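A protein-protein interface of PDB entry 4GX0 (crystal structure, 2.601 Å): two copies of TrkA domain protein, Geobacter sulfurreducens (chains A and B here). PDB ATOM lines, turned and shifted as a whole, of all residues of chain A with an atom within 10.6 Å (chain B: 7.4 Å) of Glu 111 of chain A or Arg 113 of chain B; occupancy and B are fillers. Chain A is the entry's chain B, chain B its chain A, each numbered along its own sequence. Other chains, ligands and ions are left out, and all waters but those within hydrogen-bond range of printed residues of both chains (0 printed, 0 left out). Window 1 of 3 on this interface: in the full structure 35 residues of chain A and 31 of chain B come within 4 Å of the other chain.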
ATOM      1  N   PHE A 101      21.893   3.897 -34.254  1.00  0.00           N
ATOM      2  CA  PHE A 101      23.203   4.533 -34.284  1.00  0.00           C
ATOM      3  C   PHE A 101      23.578   5.067 -32.904  1.00  0.00           C
ATOM      4  O   PHE A 101      24.747   5.059 -32.517  1.00  0.00           O
ATOM      5  CB  PHE A 101      23.220   5.665 -35.311  1.00  0.00           C
ATOM      6  CG  PHE A 101      24.527   6.397 -35.382  1.00  0.00           C
ATOM      7  CD1 PHE A 101      25.519   5.985 -36.257  1.00  0.00           C
ATOM      8  CD2 PHE A 101      24.765   7.497 -34.573  1.00  0.00           C
ATOM      9  CE1 PHE A 101      26.723   6.656 -36.326  1.00  0.00           C
ATOM     10  CE2 PHE A 101      25.969   8.172 -34.636  1.00  0.00           C
ATOM     11  CZ  PHE A 101      26.949   7.751 -35.513  1.00  0.00           C
ATOM     12  N   VAL A 102      22.578   5.533 -32.165  1.00  0.00           N
ATOM     13  CA  VAL A 102      22.790   6.019 -30.808  1.00  0.00           C
ATOM     14  C   VAL A 102      23.057   4.866 -29.840  1.00  0.00           C
ATOM     15  O   VAL A 102      23.774   5.026 -28.852  1.00  0.00           O
ATOM     16  CB  VAL A 102      21.586   6.851 -30.315  1.00  0.00           C
ATOM     17  CG1 VAL A 102      21.356   6.648 -28.824  1.00  0.00           C
ATOM     18  CG2 VAL A 102      21.788   8.322 -30.643  1.00  0.00           C
ATOM     19  N   SER A 103      22.492   3.700 -30.136  1.00  0.00           N
ATOM     20  CA  SER A 103      22.630   2.545 -29.256  1.00  0.00           C
ATOM     21  C   SER A 103      23.841   1.677 -29.597  1.00  0.00           C
ATOM     22  O   SER A 103      24.580   1.258 -28.708  1.00  0.00           O
ATOM     23  CB  SER A 103      21.353   1.703 -29.270  1.00  0.00           C
ATOM     24  OG  SER A 103      20.252   2.444 -28.775  1.00  0.00           O
ATOM     25  N   MET A 104      24.042   1.408 -30.882  1.00  0.00           N
ATOM     26  CA  MET A 104      25.139   0.549 -31.310  1.00  0.00           C
ATOM     27  C   MET A 104      26.476   1.281 -31.267  1.00  0.00           C
ATOM     28  O   MET A 104      27.520   0.672 -31.034  1.00  0.00           O
ATOM     29  CB  MET A 104      24.884   0.004 -32.720  1.00  0.00           C
ATOM     30  CG  MET A 104      25.313   0.940 -33.848  1.00  0.00           C
ATOM     31  SD  MET A 104      26.829   0.409 -34.670  1.00  0.00           S
ATOM     32  CE  MET A 104      27.132   1.795 -35.763  1.00  0.00           C
ATOM     33  N   PHE A 105      26.439   2.591 -31.485  1.00  0.00           N
ATOM     34  CA  PHE A 105      27.662   3.382 -31.554  1.00  0.00           C
ATOM     35  C   PHE A 105      27.827   4.352 -30.384  1.00  0.00           C
ATOM     36  O   PHE A 105      28.803   4.280 -29.638  1.00  0.00           O
ATOM     37  CB  PHE A 105      27.724   4.150 -32.878  1.00  0.00           C
ATOM     38  CG  PHE A 105      28.738   5.260 -32.889  1.00  0.00           C
ATOM     39  CD1 PHE A 105      28.398   6.530 -32.455  1.00  0.00           C
ATOM     40  CD2 PHE A 105      30.029   5.033 -33.332  1.00  0.00           C
ATOM     41  CE1 PHE A 105      29.326   7.556 -32.459  1.00  0.00           C
ATOM     42  CE2 PHE A 105      30.963   6.054 -33.341  1.00  0.00           C
ATOM     43  CZ  PHE A 105      30.610   7.317 -32.905  1.00  0.00           C
ATOM     44  N   LEU A 106      26.868   5.259 -30.233  1.00  0.00           N
ATOM     45  CA  LEU A 106      26.998   6.364 -29.287  1.00  0.00           C
ATOM     46  C   LEU A 106      27.139   5.913 -27.836  1.00  0.00           C
ATOM     47  O   LEU A 106      28.077   6.309 -27.146  1.00  0.00           O
ATOM     48  CB  LEU A 106      25.819   7.326 -29.427  1.00  0.00           C
ATOM     49  CG  LEU A 106      26.184   8.807 -29.395  1.00  0.00           C
ATOM     50  CD1 LEU A 106      27.696   8.991 -29.387  1.00  0.00           C
ATOM     51  CD2 LEU A 106      25.558   9.521 -30.581  1.00  0.00           C
ATOM     52  N   ALA A 107      26.202   5.091 -27.375  1.00  0.00           N
ATOM     53  CA  ALA A 107      26.219   4.620 -25.995  1.00  0.00           C
ATOM     54  C   ALA A 107      27.539   3.939 -25.627  1.00  0.00           C
ATOM     55  O   ALA A 107      28.204   4.357 -24.680  1.00  0.00           O
ATOM     56  CB  ALA A 107      25.032   3.698 -25.722  1.00  0.00           C
ATOM     57  N   PRO A 108      27.930   2.898 -26.383  1.00  0.00           N
ATOM     58  CA  PRO A 108      29.162   2.164 -26.067  1.00  0.00           C
ATOM     59  C   PRO A 108      30.372   3.083 -25.978  1.00  0.00           C
ATOM     60  O   PRO A 108      31.287   2.822 -25.199  1.00  0.00           O
ATOM     61  CB  PRO A 108      29.321   1.221 -27.264  1.00  0.00           C
ATOM     62  CG  PRO A 108      27.950   1.056 -27.804  1.00  0.00           C
ATOM     63  CD  PRO A 108      27.278   2.378 -27.597  1.00  0.00           C
ATOM     64  N   TRP A 109      30.373   4.146 -26.773  1.00  0.00           N
ATOM     65  CA  TRP A 109      31.498   5.070 -26.802  1.00  0.00           C
ATOM     66  C   TRP A 109      31.562   5.918 -25.537  1.00  0.00           C
ATOM     67  O   TRP A 109      32.589   5.958 -24.859  1.00  0.00           O
ATOM     68  CB  TRP A 109      31.422   5.964 -28.041  1.00  0.00           C
ATOM     69  CG  TRP A 109      32.522   6.976 -28.119  1.00  0.00           C
ATOM     70  CD1 TRP A 109      33.849   6.730 -28.315  1.00  0.00           C
ATOM     71  CD2 TRP A 109      32.388   8.398 -28.017  1.00  0.00           C
ATOM     72  NE1 TRP A 109      34.551   7.909 -28.335  1.00  0.00           N
ATOM     73  CE2 TRP A 109      33.677   8.949 -28.154  1.00  0.00           C
ATOM     74  CE3 TRP A 109      31.305   9.259 -27.821  1.00  0.00           C
ATOM     75  CZ2 TRP A 109      33.912  10.321 -28.101  1.00  0.00           C
ATOM     76  CZ3 TRP A 109      31.539  10.620 -27.768  1.00  0.00           C
ATOM     77  CH2 TRP A 109      32.832  11.138 -27.909  1.00  0.00           C
ATOM     78  N   ILE A 110      30.461   6.589 -25.219  1.00  0.00           N
ATOM     79  CA  ILE A 110      30.418   7.489 -24.070  1.00  0.00           C
ATOM     80  C   ILE A 110      30.502   6.745 -22.735  1.00  0.00           C
ATOM     81  O   ILE A 110      31.032   7.270 -21.756  1.00  0.00           O
ATOM     82  CB  ILE A 110      29.163   8.383 -24.099  1.00  0.00           C
ATOM     83  CG1 ILE A 110      29.081   9.130 -25.431  1.00  0.00           C
ATOM     84  CG2 ILE A 110      29.178   9.365 -22.936  1.00  0.00           C
ATOM     85  CD1 ILE A 110      27.867  10.026 -25.571  1.00  0.00           C
ATOM     86  N   GLU A 111      29.981   5.522 -22.695  1.00  0.00           N
ATOM     87  CA  GLU A 111      30.065   4.710 -21.487  1.00  0.00           C
ATOM     88  C   GLU A 111      31.509   4.318 -21.210  1.00  0.00           C
ATOM     89  O   GLU A 111      31.993   4.441 -20.086  1.00  0.00           O
ATOM     90  CB  GLU A 111      29.215   3.448 -21.620  1.00  0.00           C
ATOM     91  CG  GLU A 111      27.729   3.703 -21.759  1.00  0.00           C
ATOM     92  CD  GLU A 111      26.947   2.424 -21.978  1.00  0.00           C
ATOM     93  OE1 GLU A 111      27.478   1.342 -21.642  1.00  0.00           O
ATOM     94  OE2 GLU A 111      25.809   2.497 -22.491  1.00  0.00           O
ATOM     95  N   ARG A 112      32.195   3.850 -22.247  1.00  0.00           N
ATOM     96  CA  ARG A 112      33.550   3.333 -22.101  1.00  0.00           C
ATOM     97  C   ARG A 112      34.606   4.426 -22.246  1.00  0.00           C
ATOM     98  O   ARG A 112      35.775   4.142 -22.506  1.00  0.00           O
ATOM     99  CB  ARG A 112      33.791   2.209 -23.110  1.00  0.00           C
ATOM    100  CG  ARG A 112      32.766   1.088 -23.016  1.00  0.00           C
ATOM    101  CD  ARG A 112      32.824   0.156 -24.215  1.00  0.00           C
ATOM    102  NE  ARG A 112      31.671  -0.742 -24.254  1.00  0.00           N
ATOM    103  CZ  ARG A 112      31.418  -1.593 -25.243  1.00  0.00           C
ATOM    104  NH1 ARG A 112      32.237  -1.670 -26.283  1.00  0.00           N
ATOM    105  NH2 ARG A 112      30.342  -2.369 -25.194  1.00  0.00           N
ATOM    106  N   ARG A 113      34.192   5.677 -22.070  1.00  0.00           N
ATOM    107  CA  ARG A 113      35.126   6.797 -22.117  1.00  0.00           C
ATOM    108  C   ARG A 113      34.895   7.754 -20.950  1.00  0.00           C
ATOM    109  O   ARG A 113      35.740   8.597 -20.646  1.00  0.00           O
ATOM    110  CB  ARG A 113      35.033   7.531 -23.457  1.00  0.00           C
ATOM    111  CG  ARG A 113      36.160   8.524 -23.698  1.00  0.00           C
ATOM    112  CD  ARG A 113      36.394   8.757 -25.183  1.00  0.00           C
ATOM    113  NE  ARG A 113      36.849   7.545 -25.862  1.00  0.00           N
ATOM    114  CZ  ARG A 113      37.222   7.496 -27.138  1.00  0.00           C
ATOM    115  NH1 ARG A 113      37.196   8.592 -27.884  1.00  0.00           N
ATOM    116  NH2 ARG A 113      37.621   6.349 -27.671  1.00  0.00           N
ATOM    117  N   LEU A 114      33.747   7.613 -20.295  1.00  0.00           N
ATOM    118  CA  LEU A 114      33.438   8.398 -19.105  1.00  0.00           C
ATOM    119  C   LEU A 114      33.294   7.483 -17.896  1.00  0.00           C
ATOM    120  O   LEU A 114      33.023   7.937 -16.786  1.00  0.00           O
ATOM    121  CB  LEU A 114      32.149   9.195 -19.299  1.00  0.00           C
ATOM    122  CG  LEU A 114      32.203  10.431 -20.194  1.00  0.00           C
ATOM    123  CD1 LEU A 114      32.576  10.059 -21.618  1.00  0.00           C
ATOM    124  CD2 LEU A 114      30.868  11.153 -20.162  1.00  0.00           C
ATOM    125  N   ARG A 115      33.476   6.189 -18.126  1.00  0.00           N
ATOM    126  CA  ARG A 115      33.282   5.186 -17.090  1.00  0.00           C
ATOM    127  C   ARG A 115      34.130   3.962 -17.397  1.00  0.00           C
ATOM    128  O   ARG A 115      33.961   3.326 -18.436  1.00  0.00           O
ATOM    129  CB  ARG A 115      31.807   4.792 -17.024  1.00  0.00           C
ATOM    130  CG  ARG A 115      31.494   3.647 -16.081  1.00  0.00           C
ATOM    131  CD  ARG A 115      31.058   4.154 -14.719  1.00  0.00           C
ATOM    132  NE  ARG A 115      30.107   3.242 -14.092  1.00  0.00           N
ATOM    133  CZ  ARG A 115      29.512   3.466 -12.926  1.00  0.00           C
ATOM    134  NH1 ARG A 115      29.773   4.577 -12.251  1.00  0.00           N
ATOM    135  NH2 ARG A 115      28.657   2.579 -12.435  1.00  0.00           N
ATOM    136  N   TYR A 116      35.046   3.635 -16.491  1.00  0.00           N
ATOM    137  CA  TYR A 116      35.920   2.481 -16.674  1.00  0.00           C
ATOM    138  C   TYR A 116      35.161   1.162 -16.540  1.00  0.00           C
ATOM    139  O   TYR A 116      34.600   0.859 -15.485  1.00  0.00           O
ATOM    140  CB  TYR A 116      37.086   2.524 -15.685  1.00  0.00           C
ATOM    141  CG  TYR A 116      37.917   1.261 -15.666  1.00  0.00           C
ATOM    142  CD1 TYR A 116      37.846   0.375 -14.598  1.00  0.00           C
ATOM    143  CD2 TYR A 116      38.763   0.949 -16.721  1.00  0.00           C
ATOM    144  CE1 TYR A 116      38.603  -0.782 -14.575  1.00  0.00           C
ATOM    145  CE2 TYR A 116      39.520  -0.208 -16.709  1.00  0.00           C
ATOM    146  CZ  TYR A 116      39.438  -1.070 -15.635  1.00  0.00           C
ATOM    147  OH  TYR A 116      40.191  -2.224 -15.621  1.00  0.00           O
ATOM    148  N   HIS A 117      35.139   0.391 -17.622  1.00  0.00           N
ATOM    149  CA  HIS A 117      34.569  -0.951 -17.603  1.00  0.00           C
ATOM    150  C   HIS A 117      35.704  -1.969 -17.573  1.00  0.00           C
ATOM    151  O   HIS A 117      36.357  -2.207 -18.590  1.00  0.00           O
ATOM    152  CB  HIS A 117      33.680  -1.182 -18.828  1.00  0.00           C
ATOM    153  CG  HIS A 117      32.494  -0.272 -18.895  1.00  0.00           C
ATOM    154  ND1 HIS A 117      31.336  -0.503 -18.183  1.00  0.00           N
ATOM    155  CD2 HIS A 117      32.283   0.869 -19.593  1.00  0.00           C
ATOM    156  CE1 HIS A 117      30.465   0.457 -18.438  1.00  0.00           C
ATOM    157  NE2 HIS A 117      31.015   1.303 -19.291  1.00  0.00           N
ATOM    158  N   PRO A 118      35.944  -2.569 -16.398  1.00  0.00           N
ATOM    159  CA  PRO A 118      37.102  -3.443 -16.178  1.00  0.00           C
ATOM    160  C   PRO A 118      37.077  -4.702 -17.042  1.00  0.00           C
ATOM    161  O   PRO A 118      36.058  -5.388 -17.103  1.00  0.00           O
ATOM    162  CB  PRO A 118      36.978  -3.826 -14.697  1.00  0.00           C
ATOM    163  CG  PRO A 118      36.060  -2.805 -14.099  1.00  0.00           C
ATOM    164  CD  PRO A 118      35.111  -2.441 -15.191  1.00  0.00           C
ATOM    165  N   TYR A 160      41.398  -1.578  -8.235  1.00  0.00           N
ATOM    166  CA  TYR A 160      40.543  -0.842  -9.159  1.00  0.00           C
ATOM    167  C   TYR A 160      41.210   0.443  -9.645  1.00  0.00           C
ATOM    168  O   TYR A 160      41.360   0.657 -10.846  1.00  0.00           O
ATOM    169  CB  TYR A 160      39.215  -0.512  -8.480  1.00  0.00           C
ATOM    170  CG  TYR A 160      38.120  -0.058  -9.415  1.00  0.00           C
ATOM    171  CD1 TYR A 160      37.356  -0.979 -10.118  1.00  0.00           C
ATOM    172  CD2 TYR A 160      37.832   1.290  -9.578  1.00  0.00           C
ATOM    173  CE1 TYR A 160      36.345  -0.571 -10.969  1.00  0.00           C
ATOM    174  CE2 TYR A 160      36.823   1.710 -10.425  1.00  0.00           C
ATOM    175  CZ  TYR A 160      36.083   0.774 -11.118  1.00  0.00           C
ATOM    176  OH  TYR A 160      35.078   1.185 -11.963  1.00  0.00           O
ATOM    177  N   LEU A 164      42.398   1.415 -13.615  1.00  0.00           N
ATOM    178  CA  LEU A 164      42.028   2.613 -14.368  1.00  0.00           C
ATOM    179  C   LEU A 164      43.254   3.309 -14.942  1.00  0.00           C
ATOM    180  O   LEU A 164      43.362   3.498 -16.153  1.00  0.00           O
ATOM    181  CB  LEU A 164      41.257   3.604 -13.493  1.00  0.00           C
ATOM    182  CG  LEU A 164      39.741   3.452 -13.372  1.00  0.00           C
ATOM    183  CD1 LEU A 164      39.395   2.260 -12.502  1.00  0.00           C
ATOM    184  CD2 LEU A 164      39.130   4.721 -12.804  1.00  0.00           C
ATOM    185  N   GLU A 168      43.959   3.989 -19.111  1.00  0.00           N
ATOM    186  CA  GLU A 168      43.980   5.254 -19.839  1.00  0.00           C
ATOM    187  C   GLU A 168      45.117   5.250 -20.855  1.00  0.00           C
ATOM    188  O   GLU A 168      44.889   5.416 -22.054  1.00  0.00           O
ATOM    189  CB  GLU A 168      44.112   6.439 -18.880  1.00  0.00           C
ATOM    190  CG  GLU A 168      44.119   7.799 -19.571  1.00  0.00           C
ATOM    191  CD  GLU A 168      42.862   8.060 -20.389  1.00  0.00           C
ATOM    192  OE1 GLU A 168      41.865   7.329 -20.209  1.00  0.00           O
ATOM    193  OE2 GLU A 168      42.872   8.998 -21.215  1.00  0.00           O
ATOM    194  N   ALA B 107      17.872   9.716 -20.765  1.00  0.00           N
ATOM    195  CA  ALA B 107      18.202  10.408 -19.528  1.00  0.00           C
ATOM    196  C   ALA B 107      18.550   9.405 -18.430  1.00  0.00           C
ATOM    197  O   ALA B 107      19.608   9.506 -17.812  1.00  0.00           O
ATOM    198  CB  ALA B 107      17.056  11.317 -19.094  1.00  0.00           C
ATOM    199  N   PRO B 108      17.661   8.425 -18.187  1.00  0.00           N
ATOM    200  CA  PRO B 108      17.946   7.366 -17.213  1.00  0.00           C
ATOM    201  C   PRO B 108      19.285   6.695 -17.493  1.00  0.00           C
ATOM    202  O   PRO B 108      19.969   6.262 -16.567  1.00  0.00           O
ATOM    203  CB  PRO B 108      16.814   6.365 -17.450  1.00  0.00           C
ATOM    204  CG  PRO B 108      15.694   7.190 -17.958  1.00  0.00           C
ATOM    205  CD  PRO B 108      16.322   8.271 -18.785  1.00  0.00           C
ATOM    206  N   TRP B 109      19.644   6.611 -18.768  1.00  0.00           N
ATOM    207  CA  TRP B 109      20.893   5.985 -19.179  1.00  0.00           C
ATOM    208  C   TRP B 109      22.114   6.643 -18.536  1.00  0.00           C
ATOM    209  O   TRP B 109      22.987   5.954 -18.009  1.00  0.00           O
ATOM    210  CB  TRP B 109      21.014   5.998 -20.703  1.00  0.00           C
ATOM    211  CG  TRP B 109      22.397   5.738 -21.208  1.00  0.00           C
ATOM    212  CD1 TRP B 109      23.050   4.540 -21.234  1.00  0.00           C
ATOM    213  CD2 TRP B 109      23.294   6.698 -21.776  1.00  0.00           C
ATOM    214  NE1 TRP B 109      24.304   4.697 -21.777  1.00  0.00           N
ATOM    215  CE2 TRP B 109      24.477   6.012 -22.120  1.00  0.00           C
ATOM    216  CE3 TRP B 109      23.214   8.071 -22.028  1.00  0.00           C
ATOM    217  CZ2 TRP B 109      25.571   6.655 -22.699  1.00  0.00           C
ATOM    218  CZ3 TRP B 109      24.299   8.706 -22.603  1.00  0.00           C
ATOM    219  CH2 TRP B 109      25.462   7.999 -22.932  1.00  0.00           C
ATOM    220  N   ILE B 110      22.173   7.972 -18.576  1.00  0.00           N
ATOM    221  CA  ILE B 110      23.301   8.690 -17.992  1.00  0.00           C
ATOM    222  C   ILE B 110      23.314   8.563 -16.471  1.00  0.00           C
ATOM    223  O   ILE B 110      24.368   8.378 -15.862  1.00  0.00           O
ATOM    224  CB  ILE B 110      23.306  10.194 -18.364  1.00  0.00           C
ATOM    225  CG1 ILE B 110      22.321  10.975 -17.492  1.00  0.00           C
ATOM    226  CG2 ILE B 110      23.008  10.391 -19.842  1.00  0.00           C
ATOM    227  CD1 ILE B 110      22.572  12.462 -17.477  1.00  0.00           C
ATOM    228  N   GLU B 111      22.137   8.657 -15.862  1.00  0.00           N
ATOM    229  CA  GLU B 111      22.029   8.657 -14.410  1.00  0.00           C
ATOM    230  C   GLU B 111      22.200   7.264 -13.816  1.00  0.00           C
ATOM    231  O   GLU B 111      22.102   7.083 -12.601  1.00  0.00           O
ATOM    232  CB  GLU B 111      20.689   9.251 -13.976  1.00  0.00           C
ATOM    233  CG  GLU B 111      20.510  10.710 -14.351  1.00  0.00           C
ATOM    234  CD  GLU B 111      19.165  11.255 -13.921  1.00  0.00           C
ATOM    235  OE1 GLU B 111      18.367  10.482 -13.352  1.00  0.00           O
ATOM    236  OE2 GLU B 111      18.906  12.454 -14.151  1.00  0.00           O
ATOM    237  N   ARG B 112      22.458   6.279 -14.671  1.00  0.00           N
ATOM    238  CA  ARG B 112      22.616   4.912 -14.195  1.00  0.00           C
ATOM    239  C   ARG B 112      23.754   4.157 -14.883  1.00  0.00           C
ATOM    240  O   ARG B 112      24.009   2.996 -14.564  1.00  0.00           O
ATOM    241  CB  ARG B 112      21.304   4.134 -14.336  1.00  0.00           C
ATOM    242  CG  ARG B 112      21.205   2.949 -13.390  1.00  0.00           C
ATOM    243  CD  ARG B 112      20.611   1.728 -14.067  1.00  0.00           C
ATOM    244  NE  ARG B 112      20.923   0.507 -13.329  1.00  0.00           N
ATOM    245  CZ  ARG B 112      20.633  -0.720 -13.752  1.00  0.00           C
ATOM    246  NH1 ARG B 112      20.018  -0.894 -14.914  1.00  0.00           N
ATOM    247  NH2 ARG B 112      20.958  -1.771 -13.012  1.00  0.00           N
ATOM    248  N   ARG B 113      24.441   4.808 -15.816  1.00  0.00           N
ATOM    249  CA  ARG B 113      25.533   4.146 -16.528  1.00  0.00           C
ATOM    250  C   ARG B 113      26.792   4.999 -16.678  1.00  0.00           C
ATOM    251  O   ARG B 113      27.869   4.481 -16.982  1.00  0.00           O
ATOM    252  CB  ARG B 113      25.060   3.622 -17.888  1.00  0.00           C
ATOM    253  CG  ARG B 113      24.068   2.478 -17.769  1.00  0.00           C
ATOM    254  CD  ARG B 113      23.858   1.756 -19.086  1.00  0.00           C
ATOM    255  NE  ARG B 113      23.548   0.345 -18.869  1.00  0.00           N
ATOM    256  CZ  ARG B 113      22.336  -0.126 -18.596  1.00  0.00           C
ATOM    257  NH1 ARG B 113      21.303   0.702 -18.508  1.00  0.00           N
ATOM    258  NH2 ARG B 113      22.155  -1.427 -18.411  1.00  0.00           N
ATOM    259  N   LEU B 114      26.655   6.302 -16.462  1.00  0.00           N
ATOM    260  CA  LEU B 114      27.795   7.209 -16.519  1.00  0.00           C
ATOM    261  C   LEU B 114      28.154   7.678 -15.117  1.00  0.00           C
ATOM    262  O   LEU B 114      29.231   8.224 -14.886  1.00  0.00           O
ATOM    263  CB  LEU B 114      27.483   8.407 -17.418  1.00  0.00           C
ATOM    264  CG  LEU B 114      27.682   8.239 -18.928  1.00  0.00           C
ATOM    265  CD1 LEU B 114      27.514   6.790 -19.366  1.00  0.00           C
ATOM    266  CD2 LEU B 114      26.745   9.157 -19.710  1.00  0.00           C
ATOM    267  N   ARG B 115      27.239   7.449 -14.183  1.00  0.00           N
ATOM    268  CA  ARG B 115      27.423   7.863 -12.801  1.00  0.00           C
ATOM    269  C   ARG B 115      26.757   6.835 -11.898  1.00  0.00           C
ATOM    270  O   ARG B 115      25.530   6.794 -11.804  1.00  0.00           O
ATOM    271  CB  ARG B 115      26.784   9.234 -12.581  1.00  0.00           C
ATOM    272  CG  ARG B 115      27.376  10.038 -11.435  1.00  0.00           C
ATOM    273  CD  ARG B 115      28.718  10.637 -11.822  1.00  0.00           C
ATOM    274  NE  ARG B 115      29.147  11.671 -10.884  1.00  0.00           N
ATOM    275  CZ  ARG B 115      30.258  12.389 -11.018  1.00  0.00           C
ATOM    276  NH1 ARG B 115      31.059  12.187 -12.055  1.00  0.00           N
ATOM    277  NH2 ARG B 115      30.569  13.310 -10.115  1.00  0.00           N
ATOM    278  N   TYR B 116      27.558   6.000 -11.243  1.00  0.00           N
ATOM    279  CA  TYR B 116      27.012   4.938 -10.400  1.00  0.00           C
ATOM    280  C   TYR B 116      25.929   5.459  -9.471  1.00  0.00           C
ATOM    281  O   TYR B 116      26.141   6.413  -8.724  1.00  0.00           O
ATOM    282  CB  TYR B 116      28.104   4.252  -9.579  1.00  0.00           C
ATOM    283  CG  TYR B 116      27.547   3.326  -8.517  1.00  0.00           C
ATOM    284  CD1 TYR B 116      27.698   3.613  -7.167  1.00  0.00           C
ATOM    285  CD2 TYR B 116      26.854   2.174  -8.868  1.00  0.00           C
ATOM    286  CE1 TYR B 116      27.185   2.772  -6.194  1.00  0.00           C
ATOM    287  CE2 TYR B 116      26.337   1.328  -7.903  1.00  0.00           C
ATOM    288  CZ  TYR B 116      26.506   1.631  -6.569  1.00  0.00           C
ATOM    289  OH  TYR B 116      25.992   0.791  -5.605  1.00  0.00           O
ATOM    290  N   HIS B 117      24.766   4.821  -9.527  1.00  0.00           N
ATOM    291  CA  HIS B 117      23.642   5.195  -8.683  1.00  0.00           C
ATOM    292  C   HIS B 117      23.311   4.040  -7.749  1.00  0.00           C
ATOM    293  O   HIS B 117      22.668   3.072  -8.154  1.00  0.00           O
ATOM    294  CB  HIS B 117      22.428   5.559  -9.542  1.00  0.00           C
ATOM    295  CG  HIS B 117      21.339   6.258  -8.789  1.00  0.00           C
ATOM    296  ND1 HIS B 117      20.390   5.584  -8.051  1.00  0.00           N
ATOM    297  CD2 HIS B 117      21.048   7.575  -8.662  1.00  0.00           C
ATOM    298  CE1 HIS B 117      19.563   6.453  -7.500  1.00  0.00           C
ATOM    299  NE2 HIS B 117      19.940   7.668  -7.854  1.00  0.00           N
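The side-chain carboxylate (OE2) of Glu 111 of chain A lies within hydrogen-bond range of the indole nitrogen (NE1) of Trp 109 of chain B (2.8 Å). The backbone NH of Tyr 116 of chain B lies close to the guanidinium group of Arg 115 of chain A, at 2.8 Å.
NE2 of His 117 of chain A is in hydrogen-bond range of O of Glu 111 of chain A (3.4 Å). N of Ala 107 of chain A is in hydrogen-bond range of O of Val 102 of chain A (2.8 Å). The backbone carbonyl oxygen (O) of Ile 110 of chain B sits at hydrogen-bond distance from the backbone NH (N) of Arg 115 of chain B (3.5 Å).
Trp 109 of chain B touches Ala 107 of chain A. Trp 109 of chain B touches Ile 110 of chain A. Arg 113 of chain B touches Glu 111 of chain A. Glu 111 of chain A touches Leu 114 of chain B. Arg 113 of chain B touches Arg 115 of chain A. C of Arg 115 of chain B touches NH1 of Arg 115 of chain A, at 3.8 Å.
Printed residues of chain B within 4 Å of Ala 107 of chain A: Trp 109 (3.9 Å). Of the printed residues of chain B, Glu 111 of chain A touches Trp 109 (2.8 Å), Arg 113 (3.99 Å) and Leu 114 (3.9 Å). Arg 113 of chain A touches none of the printed residues of chain B. Printed residues of chain B within 4 Å of Arg 115 of chain A: Arg 113, Arg 115 and Tyr 116. Trp 109 of chain B touches three residues of chain A. Of the printed residues of chain A, Arg 113 of chain B touches Glu 111 and Arg 115. Printed residues of chain A within 4 Å of Leu 114 of chain B: Glu 111 (3.9 Å). Printed residues of chain A within 4 Å of Arg 115 of chain B: Arg 115 (3.8 Å). The nearest printed residue of chain B that does not touch Glu 111 of chain A is Ile 110 of chain B (7.7 Å). The nearest printed residue of chain A that does not touch Arg 115 of chain B is Leu 114 of chain A (6.4 Å).
Of the 21 printed residues of chain A, 4 touch a printed residue of chain B. Printed residues of chain B that touch a printed residue of chain A: Trp 109, Arg 113, Leu 114, Arg 115 and Tyr 116. Along chain B the printed residues that touch a printed residue of chain A span positions 109 to 116.
Ala 107 of chain A touches Trp 109 of chain B, but with the chains exchanged Trp 109 of chain A does not touch Ala 107 of chain B (14.7 Å). Glu 111 of chain A touches Leu 114 of chain B, but with the chains exchanged Leu 114 of chain A does not touch Glu 111 of chain B (10.0 Å). Arg 115 of chain B touches its own counterpart, Arg 115 of chain A. Arg 115 of chain A touches Tyr 116 of chain B, but with the chains exchanged Tyr 116 of chain A does not touch Arg 115 of chain B (9.0 Å).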
